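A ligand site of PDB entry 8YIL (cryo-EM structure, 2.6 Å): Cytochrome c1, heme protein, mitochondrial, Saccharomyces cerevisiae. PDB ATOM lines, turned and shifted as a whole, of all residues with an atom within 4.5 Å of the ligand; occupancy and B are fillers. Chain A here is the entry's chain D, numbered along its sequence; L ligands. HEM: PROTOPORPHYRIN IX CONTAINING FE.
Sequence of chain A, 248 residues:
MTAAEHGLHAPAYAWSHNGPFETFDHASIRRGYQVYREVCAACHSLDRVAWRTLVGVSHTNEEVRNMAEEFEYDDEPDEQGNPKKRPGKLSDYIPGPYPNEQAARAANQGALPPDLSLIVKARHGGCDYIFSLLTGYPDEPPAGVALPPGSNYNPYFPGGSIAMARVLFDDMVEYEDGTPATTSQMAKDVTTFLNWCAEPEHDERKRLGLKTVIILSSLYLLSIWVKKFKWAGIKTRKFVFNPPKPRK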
ATOM      1  N   VAL A  39      30.805 -15.303 -13.611  1.00  0.00           N
ATOM      2  CA  VAL A  39      29.754 -16.081 -14.255  1.00  0.00           C
ATOM      3  C   VAL A  39      29.945 -16.084 -15.774  1.00  0.00           C
ATOM      4  O   VAL A  39      29.636 -17.080 -16.439  1.00  0.00           O
ATOM      5  CB  VAL A  39      28.357 -15.547 -13.883  1.00  0.00           C
ATOM      6  CG1 VAL A  39      27.262 -16.501 -14.313  1.00  0.00           C
ATOM      7  CG2 VAL A  39      28.243 -15.273 -12.399  1.00  0.00           C
ATOM      8  N   CYS A  40      30.502 -15.006 -16.325  1.00  0.00           N
ATOM      9  CA  CYS A  40      30.385 -14.749 -17.751  1.00  0.00           C
ATOM     10  C   CYS A  40      31.647 -15.056 -18.535  1.00  0.00           C
ATOM     11  O   CYS A  40      31.557 -15.484 -19.682  1.00  0.00           O
ATOM     12  CB  CYS A  40      29.992 -13.288 -17.978  1.00  0.00           C
ATOM     13  SG  CYS A  40      29.932 -12.738 -19.693  1.00  0.00           S
ATOM     14  N   CYS A  43      32.802 -18.365 -21.020  1.00  0.00           N
ATOM     15  CA  CYS A  43      32.494 -18.641 -22.418  1.00  0.00           C
ATOM     16  C   CYS A  43      32.524 -17.430 -23.342  1.00  0.00           C
ATOM     17  O   CYS A  43      32.528 -17.627 -24.561  1.00  0.00           O
ATOM     18  CB  CYS A  43      31.114 -19.307 -22.543  1.00  0.00           C
ATOM     19  SG  CYS A  43      31.154 -21.035 -22.105  1.00  0.00           S
ATOM     20  N   HIS A  44      32.576 -16.210 -22.829  1.00  0.00           N
ATOM     21  CA  HIS A  44      32.525 -15.019 -23.662  1.00  0.00           C
ATOM     22  C   HIS A  44      33.787 -14.189 -23.504  1.00  0.00           C
ATOM     23  O   HIS A  44      34.387 -14.137 -22.430  1.00  0.00           O
ATOM     24  CB  HIS A  44      31.321 -14.167 -23.312  1.00  0.00           C
ATOM     25  CG  HIS A  44      30.048 -14.649 -23.931  1.00  0.00           C
ATOM     26  ND1 HIS A  44      29.713 -14.393 -25.241  1.00  0.00           N
ATOM     27  CD2 HIS A  44      29.032 -15.366 -23.419  1.00  0.00           C
ATOM     28  CE1 HIS A  44      28.541 -14.926 -25.500  1.00  0.00           C
ATOM     29  NE2 HIS A  44      28.114 -15.537 -24.417  1.00  0.00           N
ATOM     30  N   ASN A 108      30.535 -25.992 -26.959  1.00  0.00           N
ATOM     31  CA  ASN A 108      29.183 -25.451 -26.879  1.00  0.00           C
ATOM     32  C   ASN A 108      28.260 -26.116 -27.886  1.00  0.00           C
ATOM     33  O   ASN A 108      27.286 -25.516 -28.330  1.00  0.00           O
ATOM     34  CB  ASN A 108      29.191 -23.932 -27.089  1.00  0.00           C
ATOM     35  CG  ASN A 108      29.792 -23.193 -25.927  1.00  0.00           C
ATOM     36  OD1 ASN A 108      29.123 -22.938 -24.932  1.00  0.00           O
ATOM     37  ND2 ASN A 108      31.064 -22.843 -26.042  1.00  0.00           N
ATOM     38  N   LEU A 112      28.394 -20.944 -31.428  1.00  0.00           N
ATOM     39  CA  LEU A 112      29.487 -20.035 -31.149  1.00  0.00           C
ATOM     40  C   LEU A 112      28.980 -18.874 -30.292  1.00  0.00           C
ATOM     41  O   LEU A 112      28.164 -18.079 -30.762  1.00  0.00           O
ATOM     42  CB  LEU A 112      30.090 -19.500 -32.450  1.00  0.00           C
ATOM     43  CG  LEU A 112      31.212 -18.471 -32.389  1.00  0.00           C
ATOM     44  CD1 LEU A 112      32.419 -19.040 -31.702  1.00  0.00           C
ATOM     45  CD2 LEU A 112      31.562 -18.028 -33.784  1.00  0.00           C
ATOM     46  N   PRO A 113      29.405 -18.765 -29.031  1.00  0.00           N
ATOM     47  CA  PRO A 113      29.038 -17.603 -28.229  1.00  0.00           C
ATOM     48  C   PRO A 113      29.766 -16.364 -28.707  1.00  0.00           C
ATOM     49  O   PRO A 113      30.996 -16.384 -28.865  1.00  0.00           O
ATOM     50  CB  PRO A 113      29.471 -18.009 -26.818  1.00  0.00           C
ATOM     51  CG  PRO A 113      30.440 -19.088 -26.993  1.00  0.00           C
ATOM     52  CD  PRO A 113      30.070 -19.805 -28.243  1.00  0.00           C
ATOM     53  N   PRO A 114      29.053 -15.268 -28.960  1.00  0.00           N
ATOM     54  CA  PRO A 114      29.660 -14.087 -29.566  1.00  0.00           C
ATOM     55  C   PRO A 114      30.526 -13.286 -28.586  1.00  0.00           C
ATOM     56  O   PRO A 114      30.613 -13.578 -27.400  1.00  0.00           O
ATOM     57  CB  PRO A 114      28.447 -13.269 -30.005  1.00  0.00           C
ATOM     58  CG  PRO A 114      27.391 -13.670 -29.075  1.00  0.00           C
ATOM     59  CD  PRO A 114      27.594 -15.126 -28.856  1.00  0.00           C
ATOM     60  N   LEU A 116      31.243  -9.871 -26.519  1.00  0.00           N
ATOM     61  CA  LEU A 116      30.321  -9.001 -25.796  1.00  0.00           C
ATOM     62  C   LEU A 116      30.837  -7.574 -25.674  1.00  0.00           C
ATOM     63  O   LEU A 116      30.453  -6.851 -24.743  1.00  0.00           O
ATOM     64  CB  LEU A 116      30.016  -9.570 -24.411  1.00  0.00           C
ATOM     65  CG  LEU A 116      29.257 -10.887 -24.324  1.00  0.00           C
ATOM     66  CD1 LEU A 116      28.936 -11.185 -22.886  1.00  0.00           C
ATOM     67  CD2 LEU A 116      27.996 -10.861 -25.152  1.00  0.00           C
ATOM     68  N   ILE A 119      27.766  -5.691 -27.925  1.00  0.00           N
ATOM     69  CA  ILE A 119      26.487  -6.379 -28.021  1.00  0.00           C
ATOM     70  C   ILE A 119      25.312  -5.469 -27.672  1.00  0.00           C
ATOM     71  O   ILE A 119      24.179  -5.776 -28.040  1.00  0.00           O
ATOM     72  CB  ILE A 119      26.493  -7.645 -27.127  1.00  0.00           C
ATOM     73  CG1 ILE A 119      25.568  -8.712 -27.714  1.00  0.00           C
ATOM     74  CG2 ILE A 119      26.091  -7.354 -25.700  1.00  0.00           C
ATOM     75  CD1 ILE A 119      25.998  -9.202 -29.046  1.00  0.00           C
ATOM     76  N   ARG A 123      22.090  -4.769 -31.238  1.00  0.00           N
ATOM     77  CA  ARG A 123      20.847  -5.496 -31.038  1.00  0.00           C
ATOM     78  C   ARG A 123      19.700  -4.500 -31.022  1.00  0.00           C
ATOM     79  O   ARG A 123      19.842  -3.384 -30.509  1.00  0.00           O
ATOM     80  CB  ARG A 123      20.859  -6.296 -29.725  1.00  0.00           C
ATOM     81  CG  ARG A 123      21.729  -7.541 -29.741  1.00  0.00           C
ATOM     82  CD  ARG A 123      21.306  -8.497 -30.835  1.00  0.00           C
ATOM     83  NE  ARG A 123      22.085  -9.723 -30.870  1.00  0.00           N
ATOM     84  CZ  ARG A 123      23.249  -9.863 -31.506  1.00  0.00           C
ATOM     85  NH1 ARG A 123      23.876 -11.025 -31.494  1.00  0.00           N
ATOM     86  NH2 ARG A 123      23.777  -8.845 -32.157  1.00  0.00           N
ATOM     87  N   TYR A 129      17.054  -5.170 -24.125  1.00  0.00           N
ATOM     88  CA  TYR A 129      17.029  -6.507 -24.703  1.00  0.00           C
ATOM     89  C   TYR A 129      17.932  -7.469 -23.955  1.00  0.00           C
ATOM     90  O   TYR A 129      17.569  -8.625 -23.738  1.00  0.00           O
ATOM     91  CB  TYR A 129      17.411  -6.443 -26.176  1.00  0.00           C
ATOM     92  CG  TYR A 129      17.585  -7.804 -26.822  1.00  0.00           C
ATOM     93  CD1 TYR A 129      16.479  -8.613 -27.070  1.00  0.00           C
ATOM     94  CD2 TYR A 129      18.834  -8.270 -27.183  1.00  0.00           C
ATOM     95  CE1 TYR A 129      16.637  -9.847 -27.659  1.00  0.00           C
ATOM     96  CE2 TYR A 129      18.986  -9.502 -27.764  1.00  0.00           C
ATOM     97  CZ  TYR A 129      17.896 -10.285 -27.998  1.00  0.00           C
ATOM     98  OH  TYR A 129      18.062 -11.515 -28.584  1.00  0.00           O
ATOM     99  N   ILE A 130      19.123  -7.005 -23.542  1.00  0.00           N
ATOM    100  CA  ILE A 130      20.053  -7.866 -22.825  1.00  0.00           C
ATOM    101  C   ILE A 130      19.560  -8.167 -21.419  1.00  0.00           C
ATOM    102  O   ILE A 130      19.786  -9.259 -20.896  1.00  0.00           O
ATOM    103  CB  ILE A 130      21.468  -7.239 -22.802  1.00  0.00           C
ATOM    104  CG1 ILE A 130      21.813  -6.646 -24.167  1.00  0.00           C
ATOM    105  CG2 ILE A 130      22.506  -8.258 -22.398  1.00  0.00           C
ATOM    106  CD1 ILE A 130      22.032  -7.670 -25.241  1.00  0.00           C
ATOM    107  N   LEU A 133      16.574 -10.635 -21.849  1.00  0.00           N
ATOM    108  CA  LEU A 133      16.983 -11.943 -22.335  1.00  0.00           C
ATOM    109  C   LEU A 133      17.366 -12.867 -21.187  1.00  0.00           C
ATOM    110  O   LEU A 133      17.002 -14.043 -21.180  1.00  0.00           O
ATOM    111  CB  LEU A 133      18.145 -11.802 -23.308  1.00  0.00           C
ATOM    112  CG  LEU A 133      18.724 -13.049 -23.966  1.00  0.00           C
ATOM    113  CD1 LEU A 133      17.797 -13.575 -25.041  1.00  0.00           C
ATOM    114  CD2 LEU A 133      20.082 -12.739 -24.530  1.00  0.00           C
ATOM    115  N   LEU A 134      18.067 -12.328 -20.187  1.00  0.00           N
ATOM    116  CA  LEU A 134      18.568 -13.151 -19.096  1.00  0.00           C
ATOM    117  C   LEU A 134      17.473 -13.499 -18.100  1.00  0.00           C
ATOM    118  O   LEU A 134      17.368 -14.660 -17.671  1.00  0.00           O
ATOM    119  CB  LEU A 134      19.724 -12.449 -18.413  1.00  0.00           C
ATOM    120  CG  LEU A 134      20.838 -12.011 -19.353  1.00  0.00           C
ATOM    121  CD1 LEU A 134      21.719 -10.980 -18.681  1.00  0.00           C
ATOM    122  CD2 LEU A 134      21.661 -13.189 -19.812  1.00  0.00           C
ATOM    123  N   PHE A 157      14.280 -14.342 -28.018  1.00  0.00           N
ATOM    124  CA  PHE A 157      15.127 -14.731 -29.131  1.00  0.00           C
ATOM    125  C   PHE A 157      14.264 -15.022 -30.353  1.00  0.00           C
ATOM    126  O   PHE A 157      13.243 -15.699 -30.232  1.00  0.00           O
ATOM    127  CB  PHE A 157      15.942 -15.965 -28.779  1.00  0.00           C
ATOM    128  CG  PHE A 157      17.201 -16.103 -29.565  1.00  0.00           C
ATOM    129  CD1 PHE A 157      18.161 -15.113 -29.540  1.00  0.00           C
ATOM    130  CD2 PHE A 157      17.431 -17.231 -30.336  1.00  0.00           C
ATOM    131  CE1 PHE A 157      19.318 -15.252 -30.270  1.00  0.00           C
ATOM    132  CE2 PHE A 157      18.587 -17.354 -31.060  1.00  0.00           C
ATOM    133  CZ  PHE A 157      19.528 -16.362 -31.023  1.00  0.00           C
ATOM    134  N   ILE A 162      17.028 -21.176 -28.206  1.00  0.00           N
ATOM    135  CA  ILE A 162      18.342 -20.579 -28.038  1.00  0.00           C
ATOM    136  C   ILE A 162      19.292 -21.641 -27.501  1.00  0.00           C
ATOM    137  O   ILE A 162      18.866 -22.627 -26.892  1.00  0.00           O
ATOM    138  CB  ILE A 162      18.252 -19.323 -27.114  1.00  0.00           C
ATOM    139  CG1 ILE A 162      19.471 -18.413 -27.260  1.00  0.00           C
ATOM    140  CG2 ILE A 162      18.000 -19.715 -25.669  1.00  0.00           C
ATOM    141  CD1 ILE A 162      19.436 -17.201 -26.395  1.00  0.00           C
ATOM    142  N   ALA A 163      20.578 -21.457 -27.774  1.00  0.00           N
ATOM    143  CA  ALA A 163      21.614 -22.398 -27.363  1.00  0.00           C
ATOM    144  C   ALA A 163      22.280 -22.028 -26.042  1.00  0.00           C
ATOM    145  O   ALA A 163      23.235 -22.701 -25.648  1.00  0.00           O
ATOM    146  CB  ALA A 163      22.668 -22.524 -28.454  1.00  0.00           C
ATOM    147  N   MET A 164      21.829 -20.975 -25.374  1.00  0.00           N
ATOM    148  CA  MET A 164      22.358 -20.575 -24.071  1.00  0.00           C
ATOM    149  C   MET A 164      21.309 -20.889 -23.004  1.00  0.00           C
ATOM    150  O   MET A 164      20.143 -20.496 -23.146  1.00  0.00           O
ATOM    151  CB  MET A 164      22.693 -19.087 -24.050  1.00  0.00           C
ATOM    152  CG  MET A 164      22.773 -18.516 -22.643  1.00  0.00           C
ATOM    153  SD  MET A 164      22.944 -16.743 -22.486  1.00  0.00           S
ATOM    154  CE  MET A 164      21.767 -16.176 -23.690  1.00  0.00           C
ATOM    155  N   VAL A 167      21.854 -18.926 -16.672  1.00  0.00           N
ATOM    156  CA  VAL A 167      23.119 -18.913 -15.959  1.00  0.00           C
ATOM    157  C   VAL A 167      23.086 -18.066 -14.698  1.00  0.00           C
ATOM    158  O   VAL A 167      24.064 -18.096 -13.941  1.00  0.00           O
ATOM    159  CB  VAL A 167      24.275 -18.443 -16.868  1.00  0.00           C
ATOM    160  CG1 VAL A 167      24.257 -19.190 -18.178  1.00  0.00           C
ATOM    161  CG2 VAL A 167      24.189 -16.959 -17.105  1.00  0.00           C
ATOM    162  N   LEU A 168      22.019 -17.323 -14.440  1.00  0.00           N
ATOM    163  CA  LEU A 168      21.915 -16.493 -13.249  1.00  0.00           C
ATOM    164  C   LEU A 168      20.934 -17.110 -12.275  1.00  0.00           C
ATOM    165  O   LEU A 168      19.793 -17.422 -12.646  1.00  0.00           O
ATOM    166  CB  LEU A 168      21.466 -15.069 -13.605  1.00  0.00           C
ATOM    167  CG  LEU A 168      22.394 -14.222 -14.473  1.00  0.00           C
ATOM    168  CD1 LEU A 168      21.763 -12.887 -14.758  1.00  0.00           C
ATOM    169  CD2 LEU A 168      23.732 -14.044 -13.809  1.00  0.00           C
ATOM    170  N   VAL A 190      25.290  -6.255 -14.980  1.00  0.00           N
ATOM    171  CA  VAL A 190      26.005  -6.618 -16.196  1.00  0.00           C
ATOM    172  C   VAL A 190      25.629  -5.705 -17.347  1.00  0.00           C
ATOM    173  O   VAL A 190      26.477  -5.325 -18.159  1.00  0.00           O
ATOM    174  CB  VAL A 190      25.794  -8.098 -16.569  1.00  0.00           C
ATOM    175  CG1 VAL A 190      26.615  -8.962 -15.698  1.00  0.00           C
ATOM    176  CG2 VAL A 190      24.343  -8.488 -16.425  1.00  0.00           C
HETATM  177  CHA HEM L   1      24.709 -15.872 -26.272  1.00  0.00           C
HETATM  178  CHB HEM L   1      24.926 -12.758 -22.597  1.00  0.00           C
HETATM  179  CHC HEM L   1      26.817 -16.222 -19.804  1.00  0.00           C
HETATM  180  CHD HEM L   1      26.705 -19.298 -23.534  1.00  0.00           C
HETATM  181  C1A HEM L   1      24.611 -14.743 -25.510  1.00  0.00           C
HETATM  182  C2A HEM L   1      24.108 -13.476 -25.974  1.00  0.00           C
HETATM  183  C3A HEM L   1      24.173 -12.610 -24.972  1.00  0.00           C
HETATM  184  C4A HEM L   1      24.709 -13.304 -23.829  1.00  0.00           C
HETATM  185  CMA HEM L   1      23.745 -11.132 -25.014  1.00  0.00           C
HETATM  186  CAA HEM L   1      23.636 -13.225 -27.419  1.00  0.00           C
HETATM  187  CBA HEM L   1      22.135 -13.314 -27.591  1.00  0.00           C
HETATM  188  CGA HEM L   1      21.875 -13.126 -29.053  1.00  0.00           C
HETATM  189  O1A HEM L   1      22.686 -13.625 -29.867  1.00  0.00           O
HETATM  190  O2A HEM L   1      20.861 -12.470 -29.405  1.00  0.00           O
HETATM  191  C1B HEM L   1      25.452 -13.441 -21.529  1.00  0.00           C
HETATM  192  C2B HEM L   1      25.626 -12.885 -20.218  1.00  0.00           C
HETATM  193  C3B HEM L   1      26.151 -13.839 -19.433  1.00  0.00           C
HETATM  194  C4B HEM L   1      26.309 -15.027 -20.244  1.00  0.00           C
HETATM  195  CMB HEM L   1      25.240 -11.422 -19.928  1.00  0.00           C
HETATM  196  CAB HEM L   1      26.563 -13.886 -17.942  1.00  0.00           C
HETATM  197  CBB HEM L   1      26.331 -12.962 -17.005  1.00  0.00           C
HETATM  198  C1C HEM L   1      26.947 -17.363 -20.564  1.00  0.00           C
HETATM  199  C2C HEM L   1      27.435 -18.640 -20.107  1.00  0.00           C
HETATM  200  C3C HEM L   1      27.387 -19.502 -21.150  1.00  0.00           C
HETATM  201  C4C HEM L   1      26.880 -18.763 -22.277  1.00  0.00           C
HETATM  202  CMC HEM L   1      27.893 -18.861 -18.646  1.00  0.00           C
HETATM  203  CAC HEM L   1      27.760 -20.994 -21.322  1.00  0.00           C
HETATM  204  CBC HEM L   1      28.158 -21.854 -20.394  1.00  0.00           C
HETATM  205  C1D HEM L   1      26.134 -18.651 -24.595  1.00  0.00           C
HETATM  206  C2D HEM L   1      25.840 -19.227 -25.895  1.00  0.00           C
HETATM  207  C3D HEM L   1      25.283 -18.271 -26.639  1.00  0.00           C
HETATM  208  C4D HEM L   1      25.212 -17.067 -25.848  1.00  0.00           C
HETATM  209  CMD HEM L   1      26.100 -20.671 -26.344  1.00  0.00           C
HETATM  210  CAD HEM L   1      24.806 -18.432 -28.097  1.00  0.00           C
HETATM  211  CBD HEM L   1      23.284 -18.537 -28.124  1.00  0.00           C
HETATM  212  CGD HEM L   1      22.837 -18.759 -29.539  1.00  0.00           C
HETATM  213  O1D HEM L   1      23.479 -18.209 -30.459  1.00  0.00           O
HETATM  214  O2D HEM L   1      21.836 -19.497 -29.727  1.00  0.00           O
HETATM  215  NA  HEM L   1      24.962 -14.607 -24.183  1.00  0.00           N
HETATM  216  NB  HEM L   1      25.863 -14.746 -21.515  1.00  0.00           N
HETATM  217  NC  HEM L   1      26.620 -17.471 -21.897  1.00  0.00           N
HETATM  218  ND  HEM L   1      25.747 -17.331 -24.598  1.00  0.00           N
HETATM  219 FE   HEM L   1      25.812 -16.060 -23.056  1.00  0.00          FE
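ND1 of His 44 lies within hydrogen-bond range of O of Pro 114 (2.5 Å).
ND of the ligand lies close to NE2 of His 44. The side-chain sulfur (SD) of Met 164 lies close to a nitrogen (NA) of the ligand (3.4 Å). Val 39 touches the ligand. CB of Cys 40 touches CAB of the ligand, at 3.5 Å. Cys 43 touches the ligand. Pro 113 touches the ligand. Pro 114 touches the ligand. CD1 of Ile 130 touches CMA of the ligand (3.9 Å). CD2 of Leu 133 touches CBA of the ligand (3.7 Å). Leu 134 touches the ligand. CE1 of Phe 157 touches O2A of the ligand (3.3 Å). Ile 162 touches the ligand. CG1 of Val 167 touches CMC of the ligand (3.7 Å). 16 residues have an atom within 4 Å of the ligand: Val 39, Cys 40, Cys 43, His 44, Pro 113, Pro 114, Arg 123, Tyr 129, Ile 130, Leu 133, Leu 134, Phe 157, Ile 162, Ala 163, Met 164 and Val 167. The nearest printed residue that does not touch the ligand is Asn 108 (4.03 Å).
The backbone NH of Ala 163 is in hydrogen-bond range of an oxygen (O2D) of the ligand, at 3.0 Å. The guanidinium group (NH1) of Arg 123 lies within salt-bridge range of an oxygen (O1A) of the ligand, 3.3 Å away. OH of Tyr 129 sits at hydrogen-bond distance from O2A of the ligand (3.1 Å).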
